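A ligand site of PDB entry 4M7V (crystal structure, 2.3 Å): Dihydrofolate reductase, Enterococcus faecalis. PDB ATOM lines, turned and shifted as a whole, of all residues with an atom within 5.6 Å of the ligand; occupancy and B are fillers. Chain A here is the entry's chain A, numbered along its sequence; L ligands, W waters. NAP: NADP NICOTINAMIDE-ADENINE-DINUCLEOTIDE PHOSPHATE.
An oxygen (O2N) of the ligand lies within hydrogen-bond range of the backbone NH (N) of Ser 108 (2.4 Å). An oxygen (O2D) of the ligand is in hydrogen-bond range of the side-chain carboxylate (OD2) of Asp 133. An oxygen (O2A) of the ligand sits at hydrogen-bond distance from the backbone NH (N) of Thr 54 (3.1 Å). The side-chain hydroxyl of Thr 54 sits at hydrogen-bond distance from an oxygen (O2A) of the ligand, at 2.6 Å. The side-chain carboxylate (OE2) of Glu 113 sits at hydrogen-bond distance from a nitrogen (N7A) of the ligand (2.6 Å). A nitrogen (N3A) of the ligand lies close to the backbone NH (N) of Thr 72, 3.5 Å away. The side-chain hydroxyl (OG1) of Thr 72 is in hydrogen-bond range of an oxygen (O2X) of the ligand. The backbone NH (N) of Arg 52 lies within hydrogen-bond range of an oxygen (O4B) of the ligand, at 3.3 Å. The guanidinium group (NE) of Arg 52 lies within salt-bridge range of an oxygen (O2X) of the ligand, 2.7 Å away. N of Val 109 is in hydrogen-bond range of O1N of the ligand, 2.8 Å away. N of Gly 107 sits at hydrogen-bond distance from O2A of the ligand, at 2.8 Å. The backbone NH (N) of Ser 73 is in hydrogen-bond range of an oxygen (O3X) of the ligand (3.2 Å). An oxygen (O3X) of the ligand lies within hydrogen-bond range of the side-chain hydroxyl (OG) of Ser 73 (2.9 Å). An oxygen (O1A) of the ligand sits close to the backbone NH of Val 110 (3.4 Å). The backbone NH (N) of Ala 53 lies within hydrogen-bond range of an oxygen (O5B) of the ligand (3.4 Å).
The side-chain hydroxyl (OG1) of Thr 134 sits at hydrogen-bond distance from the side-chain carboxylate (OD1) of Asp 133 (2.7 Å). The side-chain carboxylate (OD1) of Asp 133 sits at hydrogen-bond distance from the backbone NH (N) of Glu 25 (3.0 Å). The backbone NH (N) of Gly 107 is in hydrogen-bond range of the side-chain hydroxyl (OG1) of Thr 54, 3.2 Å away. The side-chain hydroxyl of Thr 72 sits at hydrogen-bond distance from the backbone NH of Asn 74. N of Thr 72 lies within hydrogen-bond range of O of Met 85 (3.0 Å). O of Leu 50 sits at hydrogen-bond distance from N of Leu 71 (2.8 Å). The backbone carbonyl oxygen (O) of Gly 106 sits at hydrogen-bond distance from the backbone NH (N) of Gly 51, 2.7 Å away. The backbone carbonyl oxygen (O) of Thr 134 is in hydrogen-bond range of the backbone NH (N) of Ile 22 (2.8 Å).
O4B of the ligand lies close to O of Leu 71 (3.3 Å). O of His 86 lies close to N1A of the ligand (3.2 Å). Residues that only touch the ligand: Glu 25 (3.6 Å), Gly 51 (3.4 Å), Ser 87 (3.6 Å), Val 88 (3.4 Å), Gly 106 (3.8 Å) and Thr 134 (3.5 Å). Hydrophobic or aromatic side chains that line the ligand: Ala 53, Leu 71, Val 88, Val 109 and Val 110. Of the 27 residues printed, 19 come within 4 Å of the ligand. The nearest printed residue that does not touch the ligand is Gly 26 (4.3 Å).
Water W3 bridges N6A of the ligand and N of Val 88.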
ATOM      1  N   ILE A  22      10.127 -20.610  12.087  1.00  0.00           N
ATOM      2  CA  ILE A  22      10.172 -19.170  11.765  1.00  0.00           C
ATOM      3  C   ILE A  22      11.424 -18.764  11.007  1.00  0.00           C
ATOM      4  O   ILE A  22      11.476 -17.680  10.468  1.00  0.00           O
ATOM      5  CB  ILE A  22      10.067 -18.296  13.034  1.00  0.00           C
ATOM      6  CG1 ILE A  22      11.212 -18.589  14.019  1.00  0.00           C
ATOM      7  CG2 ILE A  22       8.705 -18.504  13.688  1.00  0.00           C
ATOM      8  CD1 ILE A  22      11.352 -17.569  15.127  1.00  0.00           C
ATOM      9  N   LYS A  24      15.357 -20.193   8.801  1.00  0.00           N
ATOM     10  CA  LYS A  24      16.469 -21.077   8.460  1.00  0.00           C
ATOM     11  C   LYS A  24      17.774 -20.297   8.517  1.00  0.00           C
ATOM     12  O   LYS A  24      18.144 -19.648   7.525  1.00  0.00           O
ATOM     13  CB  LYS A  24      16.292 -21.683   7.073  1.00  0.00           C
ATOM     14  CG  LYS A  24      17.126 -22.944   6.849  1.00  0.00           C
ATOM     15  CD  LYS A  24      16.852 -23.528   5.462  1.00  0.00           C
ATOM     16  CE  LYS A  24      17.257 -25.011   5.376  1.00  0.00           C
ATOM     17  NZ  LYS A  24      18.741 -25.245   5.311  1.00  0.00           N
ATOM     18  N   GLU A  25      18.454 -20.365   9.659  1.00  0.00           N
ATOM     19  CA  GLU A  25      19.713 -19.632   9.879  1.00  0.00           C
ATOM     20  C   GLU A  25      19.551 -18.166   9.511  1.00  0.00           C
ATOM     21  O   GLU A  25      20.187 -17.675   8.553  1.00  0.00           O
ATOM     22  CB  GLU A  25      20.852 -20.254   9.078  1.00  0.00           C
ATOM     23  CG  GLU A  25      21.216 -21.668   9.520  1.00  0.00           C
ATOM     24  CD  GLU A  25      22.121 -22.342   8.504  1.00  0.00           C
ATOM     25  OE1 GLU A  25      23.308 -22.564   8.831  1.00  0.00           O
ATOM     26  OE2 GLU A  25      21.636 -22.660   7.391  1.00  0.00           O
ATOM     27  N   GLY A  26      18.673 -17.484  10.243  1.00  0.00           N
ATOM     28  CA  GLY A  26      18.379 -16.083  10.004  1.00  0.00           C
ATOM     29  C   GLY A  26      17.494 -15.763   8.820  1.00  0.00           C
ATOM     30  O   GLY A  26      16.983 -14.655   8.746  1.00  0.00           O
ATOM     31  N   LEU A  50      14.819  -6.457  17.062  1.00  0.00           N
ATOM     32  CA  LEU A  50      15.358  -7.692  16.509  1.00  0.00           C
ATOM     33  C   LEU A  50      16.522  -8.214  17.366  1.00  0.00           C
ATOM     34  O   LEU A  50      17.386  -7.428  17.797  1.00  0.00           O
ATOM     35  CB  LEU A  50      15.841  -7.472  15.077  1.00  0.00           C
ATOM     36  CG  LEU A  50      14.783  -7.130  14.020  1.00  0.00           C
ATOM     37  CD1 LEU A  50      15.428  -6.899  12.641  1.00  0.00           C
ATOM     38  CD2 LEU A  50      13.733  -8.261  13.936  1.00  0.00           C
ATOM     39  N   GLY A  51      16.538  -9.520  17.619  1.00  0.00           N
ATOM     40  CA  GLY A  51      17.743 -10.153  18.111  1.00  0.00           C
ATOM     41  C   GLY A  51      18.808 -10.123  17.020  1.00  0.00           C
ATOM     42  O   GLY A  51      18.479 -10.061  15.839  1.00  0.00           O
ATOM     43  N   ARG A  52      20.083 -10.188  17.419  1.00  0.00           N
ATOM     44  CA  ARG A  52      21.193 -10.087  16.465  1.00  0.00           C
ATOM     45  C   ARG A  52      21.129 -11.121  15.333  1.00  0.00           C
ATOM     46  O   ARG A  52      21.334 -10.780  14.169  1.00  0.00           O
ATOM     47  CB  ARG A  52      22.538 -10.215  17.185  1.00  0.00           C
ATOM     48  CG  ARG A  52      23.733 -10.126  16.225  1.00  0.00           C
ATOM     49  CD  ARG A  52      25.075 -10.287  16.928  1.00  0.00           C
ATOM     50  NE  ARG A  52      25.098 -11.479  17.769  1.00  0.00           N
ATOM     51  CZ  ARG A  52      25.347 -12.713  17.314  1.00  0.00           C
ATOM     52  NH1 ARG A  52      25.605 -12.901  16.032  1.00  0.00           N
ATOM     53  NH2 ARG A  52      25.333 -13.747  18.154  1.00  0.00           N
ATOM     54  N   ALA A  53      20.847 -12.378  15.671  1.00  0.00           N
ATOM     55  CA  ALA A  53      20.817 -13.433  14.669  1.00  0.00           C
ATOM     56  C   ALA A  53      19.805 -13.104  13.570  1.00  0.00           C
ATOM     57  O   ALA A  53      20.120 -13.201  12.371  1.00  0.00           O
ATOM     58  CB  ALA A  53      20.499 -14.785  15.306  1.00  0.00           C
ATOM     59  N   THR A  54      18.620 -12.658  13.989  1.00  0.00           N
ATOM     60  CA  THR A  54      17.581 -12.248  13.038  1.00  0.00           C
ATOM     61  C   THR A  54      18.023 -11.034  12.223  1.00  0.00           C
ATOM     62  O   THR A  54      17.871 -11.010  11.004  1.00  0.00           O
ATOM     63  CB  THR A  54      16.261 -11.938  13.753  1.00  0.00           C
ATOM     64  OG1 THR A  54      15.745 -13.152  14.291  1.00  0.00           O
ATOM     65  CG2 THR A  54      15.239 -11.336  12.805  1.00  0.00           C
ATOM     66  N   PHE A  55      18.566 -10.043  12.911  1.00  0.00           N
ATOM     67  CA  PHE A  55      19.135  -8.865  12.261  1.00  0.00           C
ATOM     68  C   PHE A  55      20.136  -9.254  11.186  1.00  0.00           C
ATOM     69  O   PHE A  55      20.107  -8.744  10.072  1.00  0.00           O
ATOM     70  CB  PHE A  55      19.821  -7.972  13.294  1.00  0.00           C
ATOM     71  CG  PHE A  55      20.382  -6.690  12.704  1.00  0.00           C
ATOM     72  CD1 PHE A  55      19.550  -5.763  12.093  1.00  0.00           C
ATOM     73  CD2 PHE A  55      21.743  -6.409  12.805  1.00  0.00           C
ATOM     74  CE1 PHE A  55      20.057  -4.585  11.575  1.00  0.00           C
ATOM     75  CE2 PHE A  55      22.246  -5.232  12.278  1.00  0.00           C
ATOM     76  CZ  PHE A  55      21.413  -4.315  11.669  1.00  0.00           C
ATOM     77  N   LEU A  71      19.237  -6.251  19.567  1.00  0.00           N
ATOM     78  CA  LEU A  71      19.509  -6.706  20.913  1.00  0.00           C
ATOM     79  C   LEU A  71      20.702  -7.649  20.865  1.00  0.00           C
ATOM     80  O   LEU A  71      20.729  -8.566  20.043  1.00  0.00           O
ATOM     81  CB  LEU A  71      18.277  -7.381  21.492  1.00  0.00           C
ATOM     82  CG  LEU A  71      18.217  -7.724  22.966  1.00  0.00           C
ATOM     83  CD1 LEU A  71      18.443  -6.500  23.838  1.00  0.00           C
ATOM     84  CD2 LEU A  71      16.840  -8.317  23.225  1.00  0.00           C
ATOM     85  N   THR A  72      21.703  -7.369  21.705  1.00  0.00           N
ATOM     86  CA  THR A  72      22.915  -8.184  21.811  1.00  0.00           C
ATOM     87  C   THR A  72      23.622  -7.898  23.122  1.00  0.00           C
ATOM     88  O   THR A  72      23.523  -6.802  23.643  1.00  0.00           O
ATOM     89  CB  THR A  72      23.905  -7.955  20.643  1.00  0.00           C
ATOM     90  OG1 THR A  72      25.169  -8.541  20.977  1.00  0.00           O
ATOM     91  CG2 THR A  72      24.098  -6.484  20.358  1.00  0.00           C
ATOM     92  N   SER A  73      24.316  -8.903  23.664  1.00  0.00           N
ATOM     93  CA  SER A  73      25.087  -8.740  24.902  1.00  0.00           C
ATOM     94  C   SER A  73      26.457  -8.097  24.629  1.00  0.00           C
ATOM     95  O   SER A  73      27.082  -7.538  25.531  1.00  0.00           O
ATOM     96  CB  SER A  73      25.272 -10.087  25.603  1.00  0.00           C
ATOM     97  OG  SER A  73      26.170 -10.889  24.842  1.00  0.00           O
ATOM     98  N   ASN A  74      26.905  -8.189  23.375  1.00  0.00           N
ATOM     99  CA  ASN A  74      28.170  -7.625  22.939  1.00  0.00           C
ATOM    100  C   ASN A  74      28.172  -6.102  22.943  1.00  0.00           C
ATOM    101  O   ASN A  74      27.512  -5.460  22.103  1.00  0.00           O
ATOM    102  CB  ASN A  74      28.499  -8.139  21.538  1.00  0.00           C
ATOM    103  CG  ASN A  74      29.823  -7.600  20.998  1.00  0.00           C
ATOM    104  OD1 ASN A  74      30.610  -6.998  21.725  1.00  0.00           O
ATOM    105  ND2 ASN A  74      30.072  -7.828  19.713  1.00  0.00           N
ATOM    106  N   MET A  85      20.938  -2.199  21.710  1.00  0.00           N
ATOM    107  CA  MET A  85      20.703  -2.290  23.161  1.00  0.00           C
ATOM    108  C   MET A  85      21.075  -3.691  23.687  1.00  0.00           C
ATOM    109  O   MET A  85      21.200  -4.653  22.901  1.00  0.00           O
ATOM    110  CB  MET A  85      19.255  -1.961  23.500  1.00  0.00           C
ATOM    111  CG  MET A  85      18.854  -0.541  23.121  1.00  0.00           C
ATOM    112  SD  MET A  85      17.202  -0.096  23.692  1.00  0.00           S
ATOM    113  CE  MET A  85      16.939   1.440  22.793  1.00  0.00           C
ATOM    114  N   HIS A  86      21.243  -3.803  24.998  1.00  0.00           N
ATOM    115  CA  HIS A  86      21.969  -4.917  25.583  1.00  0.00           C
ATOM    116  C   HIS A  86      21.240  -5.686  26.699  1.00  0.00           C
ATOM    117  O   HIS A  86      21.842  -6.523  27.379  1.00  0.00           O
ATOM    118  CB  HIS A  86      23.325  -4.422  26.132  1.00  0.00           C
ATOM    119  CG  HIS A  86      24.145  -3.651  25.139  1.00  0.00           C
ATOM    120  ND1 HIS A  86      24.863  -4.262  24.129  1.00  0.00           N
ATOM    121  CD2 HIS A  86      24.381  -2.322  25.006  1.00  0.00           C
ATOM    122  CE1 HIS A  86      25.499  -3.347  23.423  1.00  0.00           C
ATOM    123  NE2 HIS A  86      25.213  -2.159  23.935  1.00  0.00           N
ATOM    124  N   SER A  87      19.952  -5.414  26.876  1.00  0.00           N
ATOM    125  CA  SER A  87      19.189  -6.153  27.859  1.00  0.00           C
ATOM    126  C   SER A  87      17.710  -5.942  27.633  1.00  0.00           C
ATOM    127  O   SER A  87      17.291  -4.938  27.033  1.00  0.00           O
ATOM    128  CB  SER A  87      19.568  -5.747  29.283  1.00  0.00           C
ATOM    129  OG  SER A  87      19.183  -4.409  29.545  1.00  0.00           O
ATOM    130  N   VAL A  88      16.917  -6.894  28.141  1.00  0.00           N
ATOM    131  CA  VAL A  88      15.472  -6.840  28.029  1.00  0.00           C
ATOM    132  C   VAL A  88      14.985  -5.599  28.713  1.00  0.00           C
ATOM    133  O   VAL A  88      14.114  -4.884  28.203  1.00  0.00           O
ATOM    134  CB  VAL A  88      14.815  -8.097  28.642  1.00  0.00           C
ATOM    135  CG1 VAL A  88      13.341  -7.848  28.913  1.00  0.00           C
ATOM    136  CG2 VAL A  88      15.001  -9.265  27.717  1.00  0.00           C
ATOM    137  N   GLY A 106      11.458 -10.592  16.366  1.00  0.00           N
ATOM    138  CA  GLY A 106      12.227 -11.828  16.519  1.00  0.00           C
ATOM    139  C   GLY A 106      13.648 -11.641  17.050  1.00  0.00           C
ATOM    140  O   GLY A 106      14.057 -10.520  17.351  1.00  0.00           O
ATOM    141  N   GLY A 107      14.398 -12.728  17.171  1.00  0.00           N
ATOM    142  CA  GLY A 107      13.910 -14.045  16.810  1.00  0.00           C
ATOM    143  C   GLY A 107      13.363 -14.825  17.984  1.00  0.00           C
ATOM    144  O   GLY A 107      12.777 -14.269  18.890  1.00  0.00           O
ATOM    145  N   SER A 108      13.593 -16.131  17.974  1.00  0.00           N
ATOM    146  CA  SER A 108      13.005 -17.031  18.968  1.00  0.00           C
ATOM    147  C   SER A 108      13.307 -16.632  20.420  1.00  0.00           C
ATOM    148  O   SER A 108      12.380 -16.417  21.200  1.00  0.00           O
ATOM    149  CB  SER A 108      13.480 -18.449  18.716  1.00  0.00           C
ATOM    150  OG  SER A 108      12.899 -19.304  19.680  1.00  0.00           O
ATOM    151  N   VAL A 109      14.583 -16.531  20.776  1.00  0.00           N
ATOM    152  CA  VAL A 109      14.985 -16.022  22.109  1.00  0.00           C
ATOM    153  C   VAL A 109      14.297 -14.707  22.501  1.00  0.00           C
ATOM    154  O   VAL A 109      13.766 -14.580  23.612  1.00  0.00           O
ATOM    155  CB  VAL A 109      16.519 -15.808  22.177  1.00  0.00           C
ATOM    156  CG1 VAL A 109      16.925 -15.065  23.445  1.00  0.00           C
ATOM    157  CG2 VAL A 109      17.233 -17.143  22.088  1.00  0.00           C
ATOM    158  N   VAL A 110      14.323 -13.737  21.596  1.00  0.00           N
ATOM    159  CA  VAL A 110      13.725 -12.446  21.857  1.00  0.00           C
ATOM    160  C   VAL A 110      12.221 -12.571  22.077  1.00  0.00           C
ATOM    161  O   VAL A 110      11.668 -11.992  23.020  1.00  0.00           O
ATOM    162  CB  VAL A 110      14.001 -11.470  20.692  1.00  0.00           C
ATOM    163  CG1 VAL A 110      13.355 -10.087  20.978  1.00  0.00           C
ATOM    164  CG2 VAL A 110      15.494 -11.320  20.486  1.00  0.00           C
ATOM    165  N   PHE A 111      11.552 -13.353  21.223  1.00  0.00           N
ATOM    166  CA  PHE A 111      10.128 -13.616  21.409  1.00  0.00           C
ATOM    167  C   PHE A 111       9.838 -14.178  22.822  1.00  0.00           C
ATOM    168  O   PHE A 111       9.016 -13.634  23.566  1.00  0.00           O
ATOM    169  CB  PHE A 111       9.622 -14.597  20.343  1.00  0.00           C
ATOM    170  CG  PHE A 111       9.383 -13.963  18.992  1.00  0.00           C
ATOM    171  CD1 PHE A 111       8.843 -12.684  18.878  1.00  0.00           C
ATOM    172  CD2 PHE A 111       9.685 -14.665  17.829  1.00  0.00           C
ATOM    173  CE1 PHE A 111       8.607 -12.126  17.614  1.00  0.00           C
ATOM    174  CE2 PHE A 111       9.470 -14.116  16.589  1.00  0.00           C
ATOM    175  CZ  PHE A 111       8.925 -12.848  16.468  1.00  0.00           C
ATOM    176  N   GLU A 113      11.407 -14.060  25.634  1.00  0.00           N
ATOM    177  CA  GLU A 113      11.665 -13.254  26.822  1.00  0.00           C
ATOM    178  C   GLU A 113      10.858 -11.968  26.806  1.00  0.00           C
ATOM    179  O   GLU A 113      10.621 -11.396  27.852  1.00  0.00           O
ATOM    180  CB  GLU A 113      13.161 -12.960  26.967  1.00  0.00           C
ATOM    181  CG  GLU A 113      13.762 -12.123  25.861  1.00  0.00           C
ATOM    182  CD  GLU A 113      15.265 -12.332  25.660  1.00  0.00           C
ATOM    183  OE1 GLU A 113      16.015 -12.663  26.632  1.00  0.00           O
ATOM    184  OE2 GLU A 113      15.711 -12.179  24.512  1.00  0.00           O
ATOM    185  N   ASP A 133      15.644 -24.360  11.008  1.00  0.00           N
ATOM    186  CA  ASP A 133      16.235 -24.751  12.290  1.00  0.00           C
ATOM    187  C   ASP A 133      15.709 -23.921  13.447  1.00  0.00           C
ATOM    188  O   ASP A 133      15.955 -24.253  14.612  1.00  0.00           O
ATOM    189  CB  ASP A 133      17.760 -24.649  12.242  1.00  0.00           C
ATOM    190  CG  ASP A 133      18.247 -23.208  12.263  1.00  0.00           C
ATOM    191  OD1 ASP A 133      17.498 -22.320  11.773  1.00  0.00           O
ATOM    192  OD2 ASP A 133      19.382 -22.973  12.762  1.00  0.00           O
ATOM    193  N   THR A 134      14.970 -22.858  13.144  1.00  0.00           N
ATOM    194  CA  THR A 134      14.516 -21.961  14.212  1.00  0.00           C
ATOM    195  C   THR A 134      12.997 -21.999  14.339  1.00  0.00           C
ATOM    196  O   THR A 134      12.268 -21.847  13.345  1.00  0.00           O
ATOM    197  CB  THR A 134      14.994 -20.505  13.967  1.00  0.00           C
ATOM    198  OG1 THR A 134      16.358 -20.519  13.508  1.00  0.00           O
ATOM    199  CG2 THR A 134      14.900 -19.685  15.237  1.00  0.00           C
HETATM  200  PA  NAP L   1      17.476 -14.073  17.745  1.00  0.00           P
HETATM  201  O1A NAP L   1      16.418 -13.985  18.874  1.00  0.00           O
HETATM  202  O2A NAP L   1      17.028 -13.353  16.510  1.00  0.00           O
HETATM  203  O5B NAP L   1      18.778 -13.378  18.240  1.00  0.00           O
HETATM  204  C5B NAP L   1      19.480 -14.012  19.261  1.00  0.00           C
HETATM  205  C4B NAP L   1      20.461 -13.098  19.910  1.00  0.00           C
HETATM  206  O4B NAP L   1      19.926 -11.770  20.360  1.00  0.00           O
HETATM  207  C3B NAP L   1      21.368 -13.610  21.006  1.00  0.00           C
HETATM  208  O3B NAP L   1      22.267 -14.605  20.761  1.00  0.00           O
HETATM  209  C2B NAP L   1      21.865 -12.333  21.547  1.00  0.00           C
HETATM  210  O2B NAP L   1      22.858 -11.678  20.875  1.00  0.00           O
HETATM  211  C1B NAP L   1      20.529 -11.640  21.707  1.00  0.00           C
HETATM  212  N9A NAP L   1      19.731 -11.315  22.836  1.00  0.00           N
HETATM  213  C8A NAP L   1      18.563 -11.890  23.101  1.00  0.00           C
HETATM  214  N7A NAP L   1      18.172 -11.440  24.396  1.00  0.00           N
HETATM  215  C5A NAP L   1      19.162 -10.598  24.881  1.00  0.00           C
HETATM  216  C6A NAP L   1      19.262  -9.916  26.072  1.00  0.00           C
HETATM  217  N6A NAP L   1      18.195 -10.041  27.030  1.00  0.00           N
HETATM  218  N1A NAP L   1      20.326  -9.160  26.295  1.00  0.00           N
HETATM  219  C2A NAP L   1      21.332  -9.064  25.361  1.00  0.00           C
HETATM  220  N3A NAP L   1      21.240  -9.748  24.165  1.00  0.00           N
HETATM  221  C4A NAP L   1      20.150 -10.499  23.954  1.00  0.00           C
HETATM  222  O3  NAP L   1      17.887 -15.560  17.409  1.00  0.00           O
HETATM  223  PN  NAP L   1      16.934 -16.818  17.540  1.00  0.00           P
HETATM  224  O1N NAP L   1      16.668 -17.100  19.052  1.00  0.00           O
HETATM  225  O2N NAP L   1      15.643 -16.620  16.785  1.00  0.00           O
HETATM  226  O5D NAP L   1      17.721 -17.990  16.868  1.00  0.00           O
HETATM  227  C5D NAP L   1      18.418 -17.687  15.690  1.00  0.00           C
HETATM  228  C4D NAP L   1      19.727 -18.397  15.478  1.00  0.00           C
HETATM  229  O4D NAP L   1      20.050 -19.561  16.324  1.00  0.00           O
HETATM  230  C3D NAP L   1      20.175 -18.760  14.077  1.00  0.00           C
HETATM  231  O3D NAP L   1      21.301 -18.176  13.551  1.00  0.00           O
HETATM  232  C2D NAP L   1      20.072 -20.244  14.007  1.00  0.00           C
HETATM  233  O2D NAP L   1      20.754 -20.927  13.024  1.00  0.00           O
HETATM  234  C1D NAP L   1      20.205 -20.717  15.446  1.00  0.00           C
HETATM  235  N1N NAP L   1      19.850 -22.016  15.959  1.00  0.00           N
HETATM  236  C2N NAP L   1      20.447 -23.290  15.618  1.00  0.00           C
HETATM  237  C3N NAP L   1      19.866 -24.600  16.155  1.00  0.00           C
HETATM  238  C7N NAP L   1      20.773 -25.756  16.162  1.00  0.00           C
HETATM  239  O7N NAP L   1      21.949 -25.562  16.455  1.00  0.00           O
HETATM  240  N7N NAP L   1      20.414 -26.893  15.401  1.00  0.00           N
HETATM  241  C4N NAP L   1      18.565 -24.616  17.001  1.00  0.00           C
HETATM  242  C5N NAP L   1      17.887 -23.234  17.146  1.00  0.00           C
HETATM  243  C6N NAP L   1      18.531 -21.973  16.550  1.00  0.00           C
HETATM  244  P2B NAP L   1      24.327 -12.070  21.229  1.00  0.00           P
HETATM  245  O1X NAP L   1      24.567 -13.546  20.786  1.00  0.00           O
HETATM  246  O2X NAP L   1      25.265 -11.137  20.416  1.00  0.00           O
HETATM  247  O3X NAP L   1      24.479 -11.911  22.728  1.00  0.00           O
HETATM  248  O   HOH W   1      28.008 -11.588  20.115  1.00  0.00           O
HETATM  249  O   HOH W   2      15.898 -26.544  16.681  1.00  0.00           O
HETATM  250  O   HOH W   3      18.390  -9.223  29.728  1.00  0.00           O
